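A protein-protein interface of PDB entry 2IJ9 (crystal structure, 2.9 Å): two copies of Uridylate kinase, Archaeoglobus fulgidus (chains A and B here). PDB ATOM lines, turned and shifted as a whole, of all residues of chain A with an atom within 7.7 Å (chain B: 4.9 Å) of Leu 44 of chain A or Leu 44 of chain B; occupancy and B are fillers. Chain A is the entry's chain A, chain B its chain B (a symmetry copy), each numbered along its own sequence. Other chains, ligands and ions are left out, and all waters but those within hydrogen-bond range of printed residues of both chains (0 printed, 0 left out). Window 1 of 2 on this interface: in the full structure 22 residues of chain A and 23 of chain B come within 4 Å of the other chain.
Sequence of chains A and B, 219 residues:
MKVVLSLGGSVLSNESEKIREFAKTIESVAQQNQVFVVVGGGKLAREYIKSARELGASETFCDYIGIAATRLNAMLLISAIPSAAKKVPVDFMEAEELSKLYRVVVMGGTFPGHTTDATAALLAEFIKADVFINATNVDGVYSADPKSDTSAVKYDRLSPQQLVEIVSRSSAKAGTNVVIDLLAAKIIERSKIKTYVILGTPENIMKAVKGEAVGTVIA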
ATOM      1  N   SER A  10     -11.471   4.163   7.377  1.00  0.00           N
ATOM      2  CA  SER A  10     -10.639   3.416   8.341  1.00  0.00           C
ATOM      3  C   SER A  10     -11.522   2.810   9.432  1.00  0.00           C
ATOM      4  O   SER A  10     -11.310   1.679   9.857  1.00  0.00           O
ATOM      5  CB  SER A  10      -9.527   4.266   9.006  1.00  0.00           C
ATOM      6  OG  SER A  10      -8.672   4.914   8.075  1.00  0.00           O
ATOM      7  N   SER A  13     -13.641  -0.674   8.272  1.00  0.00           N
ATOM      8  CA  SER A  13     -13.485  -1.370   6.974  1.00  0.00           C
ATOM      9  C   SER A  13     -13.684  -2.899   7.008  1.00  0.00           C
ATOM     10  O   SER A  13     -12.732  -3.662   7.193  1.00  0.00           O
ATOM     11  CB  SER A  13     -12.152  -1.009   6.291  1.00  0.00           C
ATOM     12  OG  SER A  13     -12.301   0.099   5.415  1.00  0.00           O
ATOM     13  N   ASN A  14     -14.938  -3.310   6.820  1.00  0.00           N
ATOM     14  CA  ASN A  14     -15.349  -4.714   6.588  1.00  0.00           C
ATOM     15  C   ASN A  14     -14.820  -5.851   7.504  1.00  0.00           C
ATOM     16  O   ASN A  14     -14.598  -6.976   7.047  1.00  0.00           O
ATOM     17  CB  ASN A  14     -15.278  -5.093   5.082  1.00  0.00           C
ATOM     18  CG  ASN A  14     -13.939  -4.734   4.422  1.00  0.00           C
ATOM     19  OD1 ASN A  14     -12.889  -5.268   4.780  1.00  0.00           O
ATOM     20  ND2 ASN A  14     -13.985  -3.836   3.439  1.00  0.00           N
ATOM     21  N   GLY A  40     -18.359   6.448   5.498  1.00  0.00           N
ATOM     22  CA  GLY A  40     -17.438   6.941   4.473  1.00  0.00           C
ATOM     23  C   GLY A  40     -16.872   5.805   3.649  1.00  0.00           C
ATOM     24  O   GLY A  40     -17.116   4.630   3.942  1.00  0.00           O
ATOM     25  N   GLY A  41     -16.089   6.158   2.636  1.00  0.00           N
ATOM     26  CA  GLY A  41     -15.576   5.188   1.679  1.00  0.00           C
ATOM     27  C   GLY A  41     -14.497   4.214   2.123  1.00  0.00           C
ATOM     28  O   GLY A  41     -14.355   3.147   1.524  1.00  0.00           O
ATOM     29  N   GLY A  42     -13.721   4.586   3.140  1.00  0.00           N
ATOM     30  CA  GLY A  42     -12.692   3.707   3.711  1.00  0.00           C
ATOM     31  C   GLY A  42     -11.669   3.215   2.714  1.00  0.00           C
ATOM     32  O   GLY A  42     -11.352   3.906   1.743  1.00  0.00           O
ATOM     33  N   LYS A  43     -11.165   2.010   2.943  1.00  0.00           N
ATOM     34  CA  LYS A  43     -10.238   1.385   2.009  1.00  0.00           C
ATOM     35  C   LYS A  43     -10.895   1.388   0.642  1.00  0.00           C
ATOM     36  O   LYS A  43     -10.350   1.934  -0.322  1.00  0.00           O
ATOM     37  CB  LYS A  43      -9.915  -0.047   2.450  1.00  0.00           C
ATOM     38  CG  LYS A  43      -8.654  -0.655   1.828  1.00  0.00           C
ATOM     39  CD  LYS A  43      -8.414  -2.112   2.286  1.00  0.00           C
ATOM     40  CE  LYS A  43      -7.862  -2.208   3.718  1.00  0.00           C
ATOM     41  NZ  LYS A  43      -7.100  -3.475   3.972  1.00  0.00           N
ATOM     42  N   LEU A  44     -12.103   0.831   0.610  1.00  0.00           N
ATOM     43  CA  LEU A  44     -12.883   0.645  -0.596  1.00  0.00           C
ATOM     44  C   LEU A  44     -12.862   1.836  -1.539  1.00  0.00           C
ATOM     45  O   LEU A  44     -12.559   1.690  -2.728  1.00  0.00           O
ATOM     46  CB  LEU A  44     -14.317   0.323  -0.217  1.00  0.00           C
ATOM     47  CG  LEU A  44     -15.174  -0.070  -1.403  1.00  0.00           C
ATOM     48  CD1 LEU A  44     -14.522  -1.237  -2.108  1.00  0.00           C
ATOM     49  CD2 LEU A  44     -16.559  -0.416  -0.909  1.00  0.00           C
ATOM     50  N   ALA A  45     -13.191   3.010  -1.012  1.00  0.00           N
ATOM     51  CA  ALA A  45     -13.252   4.203  -1.855  1.00  0.00           C
ATOM     52  C   ALA A  45     -11.875   4.614  -2.280  1.00  0.00           C
ATOM     53  O   ALA A  45     -11.653   4.887  -3.450  1.00  0.00           O
ATOM     54  CB  ALA A  45     -13.902   5.333  -1.143  1.00  0.00           C
ATOM     55  N   ARG A  46     -10.953   4.651  -1.320  1.00  0.00           N
ATOM     56  CA  ARG A  46      -9.590   5.063  -1.593  1.00  0.00           C
ATOM     57  C   ARG A  46      -9.020   4.223  -2.725  1.00  0.00           C
ATOM     58  O   ARG A  46      -8.480   4.762  -3.698  1.00  0.00           O
ATOM     59  CB  ARG A  46      -8.729   4.932  -0.341  1.00  0.00           C
ATOM     60  CG  ARG A  46      -9.014   5.989   0.699  1.00  0.00           C
ATOM     61  CD  ARG A  46      -8.142   5.833   1.926  1.00  0.00           C
ATOM     62  NE  ARG A  46      -8.659   6.647   3.025  1.00  0.00           N
ATOM     63  CZ  ARG A  46      -9.191   6.161   4.145  1.00  0.00           C
ATOM     64  NH1 ARG A  46      -9.273   4.851   4.342  1.00  0.00           N
ATOM     65  NH2 ARG A  46      -9.626   6.990   5.083  1.00  0.00           N
ATOM     66  N   GLU A  47      -9.196   2.908  -2.588  1.00  0.00           N
ATOM     67  CA  GLU A  47      -8.718   1.907  -3.522  1.00  0.00           C
ATOM     68  C   GLU A  47      -9.280   2.203  -4.893  1.00  0.00           C
ATOM     69  O   GLU A  47      -8.533   2.323  -5.869  1.00  0.00           O
ATOM     70  CB  GLU A  47      -9.197   0.536  -3.031  1.00  0.00           C
ATOM     71  CG  GLU A  47      -8.482  -0.710  -3.555  1.00  0.00           C
ATOM     72  CD  GLU A  47      -8.985  -1.983  -2.855  1.00  0.00           C
ATOM     73  OE1 GLU A  47      -9.030  -3.050  -3.508  1.00  0.00           O
ATOM     74  OE2 GLU A  47      -9.350  -1.913  -1.652  1.00  0.00           O
ATOM     75  N   TYR A  48     -10.599   2.346  -4.966  1.00  0.00           N
ATOM     76  CA  TYR A  48     -11.253   2.412  -6.255  1.00  0.00           C
ATOM     77  C   TYR A  48     -11.014   3.722  -6.986  1.00  0.00           C
ATOM     78  O   TYR A  48     -10.895   3.744  -8.211  1.00  0.00           O
ATOM     79  CB  TYR A  48     -12.732   2.083  -6.135  1.00  0.00           C
ATOM     80  CG  TYR A  48     -13.007   0.608  -6.288  1.00  0.00           C
ATOM     81  CD1 TYR A  48     -12.825  -0.262  -5.219  1.00  0.00           C
ATOM     82  CD2 TYR A  48     -13.438   0.078  -7.506  1.00  0.00           C
ATOM     83  CE1 TYR A  48     -13.087  -1.614  -5.350  1.00  0.00           C
ATOM     84  CE2 TYR A  48     -13.696  -1.273  -7.642  1.00  0.00           C
ATOM     85  CZ  TYR A  48     -13.514  -2.107  -6.562  1.00  0.00           C
ATOM     86  OH  TYR A  48     -13.766  -3.440  -6.684  1.00  0.00           O
ATOM     87  N   ILE A  49     -10.949   4.809  -6.228  1.00  0.00           N
ATOM     88  CA  ILE A  49     -10.654   6.118  -6.792  1.00  0.00           C
ATOM     89  C   ILE A  49      -9.233   6.083  -7.334  1.00  0.00           C
ATOM     90  O   ILE A  49      -8.996   6.446  -8.491  1.00  0.00           O
ATOM     91  CB  ILE A  49     -10.777   7.225  -5.749  1.00  0.00           C
ATOM     92  CG1 ILE A  49     -12.224   7.359  -5.298  1.00  0.00           C
ATOM     93  CG2 ILE A  49     -10.351   8.539  -6.346  1.00  0.00           C
ATOM     94  CD1 ILE A  49     -12.370   8.036  -3.973  1.00  0.00           C
ATOM     95  N   LYS A  50      -8.306   5.619  -6.495  1.00  0.00           N
ATOM     96  CA  LYS A  50      -6.929   5.365  -6.906  1.00  0.00           C
ATOM     97  C   LYS A  50      -6.924   4.672  -8.276  1.00  0.00           C
ATOM     98  O   LYS A  50      -6.430   5.240  -9.261  1.00  0.00           O
ATOM     99  CB  LYS A  50      -6.217   4.512  -5.847  1.00  0.00           C
ATOM    100  CG  LYS A  50      -4.682   4.551  -5.835  1.00  0.00           C
ATOM    101  CD  LYS A  50      -4.113   3.318  -5.101  1.00  0.00           C
ATOM    102  CE  LYS A  50      -2.597   3.263  -5.130  1.00  0.00           C
ATOM    103  NZ  LYS A  50      -2.083   1.903  -4.791  1.00  0.00           N
ATOM    104  N   ILE A  65     -17.894   7.216  -8.137  1.00  0.00           N
ATOM    105  CA  ILE A  65     -17.284   5.997  -7.620  1.00  0.00           C
ATOM    106  C   ILE A  65     -17.184   6.046  -6.108  1.00  0.00           C
ATOM    107  O   ILE A  65     -17.478   5.059  -5.413  1.00  0.00           O
ATOM    108  CB  ILE A  65     -15.876   5.776  -8.229  1.00  0.00           C
ATOM    109  CG1 ILE A  65     -16.016   5.501  -9.724  1.00  0.00           C
ATOM    110  CG2 ILE A  65     -15.127   4.667  -7.491  1.00  0.00           C
ATOM    111  CD1 ILE A  65     -15.018   4.537 -10.291  1.00  0.00           C
ATOM    112  N   GLY A  66     -16.779   7.206  -5.605  1.00  0.00           N
ATOM    113  CA  GLY A  66     -16.592   7.374  -4.176  1.00  0.00           C
ATOM    114  C   GLY A  66     -17.914   7.227  -3.446  1.00  0.00           C
ATOM    115  O   GLY A  66     -18.010   6.522  -2.427  1.00  0.00           O
ATOM    116  N   ALA A  68     -20.621   5.770  -4.471  1.00  0.00           N
ATOM    117  CA  ALA A  68     -20.986   4.370  -4.631  1.00  0.00           C
ATOM    118  C   ALA A  68     -20.408   3.570  -3.487  1.00  0.00           C
ATOM    119  O   ALA A  68     -21.131   2.864  -2.752  1.00  0.00           O
ATOM    120  CB  ALA A  68     -20.471   3.833  -5.953  1.00  0.00           C
ATOM    121  N   ALA A  69     -19.101   3.722  -3.331  1.00  0.00           N
ATOM    122  CA  ALA A  69     -18.360   2.979  -2.346  1.00  0.00           C
ATOM    123  C   ALA A  69     -18.893   3.258  -0.946  1.00  0.00           C
ATOM    124  O   ALA A  69     -18.999   2.342  -0.115  1.00  0.00           O
ATOM    125  CB  ALA A  69     -16.859   3.298  -2.462  1.00  0.00           C
ATOM    126  N   THR A  70     -19.225   4.518  -0.680  1.00  0.00           N
ATOM    127  CA  THR A  70     -19.783   4.868   0.645  1.00  0.00           C
ATOM    128  C   THR A  70     -21.103   4.110   0.847  1.00  0.00           C
ATOM    129  O   THR A  70     -21.314   3.472   1.867  1.00  0.00           O
ATOM    130  CB  THR A  70     -20.017   6.410   0.854  1.00  0.00           C
ATOM    131  OG1 THR A  70     -20.878   6.916  -0.178  1.00  0.00           O
ATOM    132  CG2 THR A  70     -18.724   7.168   0.844  1.00  0.00           C
ATOM    133  N   ARG A  71     -21.951   4.155  -0.174  1.00  0.00           N
ATOM    134  CA  ARG A  71     -23.247   3.522  -0.154  1.00  0.00           C
ATOM    135  C   ARG A  71     -23.125   2.051   0.121  1.00  0.00           C
ATOM    136  O   ARG A  71     -23.960   1.497   0.822  1.00  0.00           O
ATOM    137  CB  ARG A  71     -23.932   3.704  -1.500  1.00  0.00           C
ATOM    138  CG  ARG A  71     -24.009   5.150  -1.976  1.00  0.00           C
ATOM    139  CD  ARG A  71     -25.317   5.816  -1.578  1.00  0.00           C
ATOM    140  NE  ARG A  71     -25.382   7.198  -2.035  1.00  0.00           N
ATOM    141  CZ  ARG A  71     -25.633   7.563  -3.287  1.00  0.00           C
ATOM    142  NH1 ARG A  71     -25.841   6.643  -4.222  1.00  0.00           N
ATOM    143  NH2 ARG A  71     -25.660   8.853  -3.607  1.00  0.00           N
ATOM    144  N   LEU A  72     -22.088   1.424  -0.431  1.00  0.00           N
ATOM    145  CA  LEU A  72     -21.864   0.000  -0.228  1.00  0.00           C
ATOM    146  C   LEU A  72     -21.516  -0.301   1.230  1.00  0.00           C
ATOM    147  O   LEU A  72     -22.102  -1.181   1.868  1.00  0.00           O
ATOM    148  CB  LEU A  72     -20.781  -0.509  -1.184  1.00  0.00           C
ATOM    149  CG  LEU A  72     -20.535  -2.014  -1.278  1.00  0.00           C
ATOM    150  CD1 LEU A  72     -21.841  -2.809  -1.171  1.00  0.00           C
ATOM    151  CD2 LEU A  72     -19.820  -2.312  -2.589  1.00  0.00           C
ATOM    152  N   ASN A  73     -20.567   0.447   1.759  1.00  0.00           N
ATOM    153  CA  ASN A  73     -20.196   0.323   3.159  1.00  0.00           C
ATOM    154  C   ASN A  73     -21.386   0.529   4.057  1.00  0.00           C
ATOM    155  O   ASN A  73     -21.536  -0.137   5.072  1.00  0.00           O
ATOM    156  CB  ASN A  73     -19.139   1.357   3.492  1.00  0.00           C
ATOM    157  CG  ASN A  73     -17.810   1.023   2.883  1.00  0.00           C
ATOM    158  OD1 ASN A  73     -17.162   1.866   2.269  1.00  0.00           O
ATOM    159  ND2 ASN A  73     -17.406  -0.227   3.027  1.00  0.00           N
ATOM    160  N   ALA A  74     -22.233   1.470   3.661  1.00  0.00           N
ATOM    161  CA  ALA A  74     -23.445   1.765   4.381  1.00  0.00           C
ATOM    162  C   ALA A  74     -24.343   0.521   4.383  1.00  0.00           C
ATOM    163  O   ALA A  74     -24.787   0.084   5.454  1.00  0.00           O
ATOM    164  CB  ALA A  74     -24.143   2.964   3.765  1.00  0.00           C
ATOM    165  N   GLY B  41     -19.303  -9.478  -9.750  1.00  0.00           N
ATOM    166  CA  GLY B  41     -18.895  -8.963  -8.445  1.00  0.00           C
ATOM    167  C   GLY B  41     -17.460  -9.206  -8.005  1.00  0.00           C
ATOM    168  O   GLY B  41     -16.910  -8.419  -7.220  1.00  0.00           O
ATOM    169  N   GLY B  42     -16.870 -10.303  -8.488  1.00  0.00           N
ATOM    170  CA  GLY B  42     -15.491 -10.667  -8.177  1.00  0.00           C
ATOM    171  C   GLY B  42     -15.244 -10.843  -6.689  1.00  0.00           C
ATOM    172  O   GLY B  42     -16.132 -11.275  -5.928  1.00  0.00           O
ATOM    173  N   LYS B  43     -14.030 -10.488  -6.277  1.00  0.00           N
ATOM    174  CA  LYS B  43     -13.623 -10.569  -4.878  1.00  0.00           C
ATOM    175  C   LYS B  43     -14.611  -9.725  -4.081  1.00  0.00           C
ATOM    176  O   LYS B  43     -15.285 -10.212  -3.167  1.00  0.00           O
ATOM    177  CB  LYS B  43     -12.187 -10.032  -4.710  1.00  0.00           C
ATOM    178  CG  LYS B  43     -11.475 -10.463  -3.426  1.00  0.00           C
ATOM    179  CD  LYS B  43     -10.078  -9.828  -3.280  1.00  0.00           C
ATOM    180  CE  LYS B  43      -8.998 -10.558  -4.093  1.00  0.00           C
ATOM    181  NZ  LYS B  43      -7.605 -10.279  -3.597  1.00  0.00           N
ATOM    182  N   LEU B  44     -14.718  -8.472  -4.506  1.00  0.00           N
ATOM    183  CA  LEU B  44     -15.576  -7.470  -3.900  1.00  0.00           C
ATOM    184  C   LEU B  44     -16.946  -7.995  -3.465  1.00  0.00           C
ATOM    185  O   LEU B  44     -17.303  -7.912  -2.288  1.00  0.00           O
ATOM    186  CB  LEU B  44     -15.751  -6.307  -4.872  1.00  0.00           C
ATOM    187  CG  LEU B  44     -16.448  -5.090  -4.276  1.00  0.00           C
ATOM    188  CD1 LEU B  44     -15.661  -4.628  -3.084  1.00  0.00           C
ATOM    189  CD2 LEU B  44     -16.579  -3.983  -5.300  1.00  0.00           C
ATOM    190  N   ALA B  45     -17.715  -8.530  -4.409  1.00  0.00           N
ATOM    191  CA  ALA B  45     -19.017  -9.058  -4.062  1.00  0.00           C
ATOM    192  C   ALA B  45     -18.882 -10.219  -3.095  1.00  0.00           C
ATOM    193  O   ALA B  45     -19.533 -10.214  -2.043  1.00  0.00           O
ATOM    194  CB  ALA B  45     -19.776  -9.469  -5.282  1.00  0.00           C
ATOM    195  N   ARG B  46     -18.015 -11.184  -3.436  1.00  0.00           N
ATOM    196  CA  ARG B  46     -17.846 -12.407  -2.632  1.00  0.00           C
ATOM    197  C   ARG B  46     -17.576 -12.023  -1.190  1.00  0.00           C
ATOM    198  O   ARG B  46     -18.244 -12.487  -0.258  1.00  0.00           O
ATOM    199  CB  ARG B  46     -16.710 -13.285  -3.183  1.00  0.00           C
ATOM    200  CG  ARG B  46     -17.079 -14.025  -4.471  1.00  0.00           C
ATOM    201  CD  ARG B  46     -15.942 -14.890  -5.009  1.00  0.00           C
ATOM    202  NE  ARG B  46     -16.188 -15.316  -6.392  1.00  0.00           N
ATOM    203  CZ  ARG B  46     -15.457 -14.942  -7.442  1.00  0.00           C
ATOM    204  NH1 ARG B  46     -14.414 -14.135  -7.284  1.00  0.00           N
ATOM    205  NH2 ARG B  46     -15.759 -15.387  -8.654  1.00  0.00           N
ATOM    206  N   GLU B  47     -16.607 -11.128  -1.051  1.00  0.00           N
ATOM    207  CA  GLU B  47     -16.172 -10.556   0.211  1.00  0.00           C
ATOM    208  C   GLU B  47     -17.337  -9.931   0.976  1.00  0.00           C
ATOM    209  O   GLU B  47     -17.588 -10.276   2.127  1.00  0.00           O
ATOM    210  CB  GLU B  47     -15.138  -9.481  -0.112  1.00  0.00           C
ATOM    211  CG  GLU B  47     -14.191  -9.098   0.986  1.00  0.00           C
ATOM    212  CD  GLU B  47     -13.149  -8.092   0.503  1.00  0.00           C
ATOM    213  OE1 GLU B  47     -12.711  -7.244   1.313  1.00  0.00           O
ATOM    214  OE2 GLU B  47     -12.776  -8.142  -0.691  1.00  0.00           O
ATOM    215  N   TYR B  48     -18.061  -9.028   0.315  1.00  0.00           N
ATOM    216  CA  TYR B  48     -19.112  -8.259   0.976  1.00  0.00           C
ATOM    217  C   TYR B  48     -20.340  -9.055   1.362  1.00  0.00           C
ATOM    218  O   TYR B  48     -20.857  -8.871   2.474  1.00  0.00           O
ATOM    219  CB  TYR B  48     -19.496  -7.025   0.161  1.00  0.00           C
ATOM    220  CG  TYR B  48     -18.617  -5.851   0.514  1.00  0.00           C
ATOM    221  CD1 TYR B  48     -17.363  -5.703  -0.068  1.00  0.00           C
ATOM    222  CD2 TYR B  48     -19.017  -4.913   1.468  1.00  0.00           C
ATOM    223  CE1 TYR B  48     -16.535  -4.640   0.260  1.00  0.00           C
ATOM    224  CE2 TYR B  48     -18.187  -3.838   1.812  1.00  0.00           C
ATOM    225  CZ  TYR B  48     -16.943  -3.719   1.197  1.00  0.00           C
ATOM    226  OH  TYR B  48     -16.090  -2.686   1.496  1.00  0.00           O
ATOM    227  N   ILE B  49     -20.803  -9.913   0.449  1.00  0.00           N
ATOM    228  CA  ILE B  49     -21.859 -10.869   0.751  1.00  0.00           C
ATOM    229  C   ILE B  49     -21.443 -11.771   1.925  1.00  0.00           C
ATOM    230  O   ILE B  49     -22.195 -11.921   2.892  1.00  0.00           O
ATOM    231  CB  ILE B  49     -22.177 -11.722  -0.470  1.00  0.00           C
ATOM    232  CG1 ILE B  49     -22.620 -10.819  -1.626  1.00  0.00           C
ATOM    233  CG2 ILE B  49     -23.254 -12.770  -0.133  1.00  0.00           C
ATOM    234  CD1 ILE B  49     -22.506 -11.464  -3.004  1.00  0.00           C
ATOM    235  N   ALA B  69     -21.875  -4.020  -5.708  1.00  0.00           N
ATOM    236  CA  ALA B  69     -20.507  -4.401  -6.030  1.00  0.00           C
ATOM    237  C   ALA B  69     -20.246  -4.525  -7.536  1.00  0.00           C
ATOM    238  O   ALA B  69     -19.285  -3.939  -8.058  1.00  0.00           O
ATOM    239  CB  ALA B  69     -20.174  -5.698  -5.326  1.00  0.00           C
ATOM    240  N   LEU B  72     -20.012  -1.202  -9.070  1.00  0.00           N
ATOM    241  CA  LEU B  72     -18.757  -0.553  -8.709  1.00  0.00           C
ATOM    242  C   LEU B  72     -17.592  -1.021  -9.591  1.00  0.00           C
ATOM    243  O   LEU B  72     -16.842  -0.207 -10.126  1.00  0.00           O
ATOM    244  CB  LEU B  72     -18.440  -0.806  -7.233  1.00  0.00           C
ATOM    245  CG  LEU B  72     -17.330   0.043  -6.623  1.00  0.00           C
ATOM    246  CD1 LEU B  72     -17.247   1.466  -7.194  1.00  0.00           C
ATOM    247  CD2 LEU B  72     -17.549   0.086  -5.144  1.00  0.00           C
ATOM    248  N   ASN B  73     -17.453  -2.334  -9.737  1.00  0.00           N
ATOM    249  CA  ASN B  73     -16.512  -2.874 -10.685  1.00  0.00           C
ATOM    250  C   ASN B  73     -16.743  -2.284 -12.061  1.00  0.00           C
ATOM    251  O   ASN B  73     -15.799  -1.911 -12.762  1.00  0.00           O
ATOM    252  CB  ASN B  73     -16.648  -4.383 -10.735  1.00  0.00           C
ATOM    253  CG  ASN B  73     -16.216  -5.026  -9.461  1.00  0.00           C
ATOM    254  OD1 ASN B  73     -16.815  -5.994  -9.001  1.00  0.00           O
ATOM    255  ND2 ASN B  73     -15.167  -4.478  -8.862  1.00  0.00           N
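O of Gly 40 of chain A sits close to OD1 of Asn 73 of chain A, at 3.2 Å.
O of Gly 41 of chain A sits close to OD1 of Asn 73 of chain A, at 3.2 Å.
The side-chain amide oxygen of Asn 73 of chain A lies close to the backbone carbonyl oxygen of Ala 69 of chain A (3.0 Å).
The side-chain amide oxygen (OD1) of Asn 73 of chain B lies close to the backbone carbonyl oxygen (O) of Gly 41 of chain B.
OD1 of Asn 73 of chain B lies close to O of Ala 69 of chain B.
The side-chain hydroxyl (OH) of Tyr 48 of chain B sits at hydrogen-bond distance from the side-chain amide nitrogen (ND2) of Asn 14 of chain A (3.1 Å).
The side-chain hydroxyl (OH) of Tyr 48 of chain A sits at hydrogen-bond distance from the side-chain amide nitrogen (ND2) of Asn 73 of chain B (2.8 Å).
The side-chain hydroxyl of Tyr 48 of chain B is in hydrogen-bond range of the side-chain amide nitrogen of Asn 73 of chain A (3.2 Å).
Asn 14 of chain A touches Glu 47 of chain B (OD1 to OE1, 3.99 Å).
Leu 44 of chain A touches Leu 44 of chain B (CD1 to CD1, 3.7 Å).
Leu 44 of chain A touches Tyr 48 of chain B.
Leu 44 of chain B touches Tyr 48 of chain A.
CG of Leu 72 of chain B touches CD2 of Tyr 48 of chain A, 3.99 Å away.
CG2 of Ile 65 of chain A touches CD1 of Leu 72 of chain B (3.9 Å).
Leu 44 of chain A touches its own counterpart, Leu 44 of chain B.
Leu 44 of chain A touches Tyr 48 of chain B, and with the chains exchanged Tyr 48 of chain A touches Leu 44 of chain B.
Tyr 48 of chain A touches Leu 72 of chain B, but with the chains exchanged Leu 72 of chain A does not touch Tyr 48 of chain B (4.3 Å).
Tyr 48 of chain A touches Asn 73 of chain B, and with the chains exchanged Asn 73 of chain A touches Tyr 48 of chain B.
Of the 12 printed residues of chain B, 5 touch a printed residue of chain A.
Printed residues of chain B that touch a printed residue of chain A: Leu 44, Glu 47, Tyr 48, Leu 72 and Asn 73.
Hydrophobic or aromatic side chains of chain B within 4 Å of the printed part of chain A: Leu 44, Tyr 48 and Leu 72.
Of the 23 printed residues of chain A, 5 touch a printed residue of chain B.
Hydrophobic or aromatic side chains of chain A that line the printed part of chain B: Leu 44, Tyr 48 and Ile 65.
Among the printed residues, no Asp or Glu carboxylate lies within 4 Å of a Lys or Arg side-chain nitrogen of the other chain.
Of chain A, only Leu 44 (3.7 Å) and Tyr 48 (3.2 Å) come within 4 Å of Leu 44 of chain B.
Of the printed residues of chain B, Asn 73 of chain A touches Tyr 48 (3.2 Å).
Printed residues of chain A within 4 Å of Asn 73 of chain B: Tyr 48.
Of the printed residues of chain B, Tyr 48 of chain A touches Leu 44, Leu 72 and Asn 73.
Glu 47 of chain A touches none of the printed residues of chain B.
Lys 43 of chain A touches none of the printed residues of chain B.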
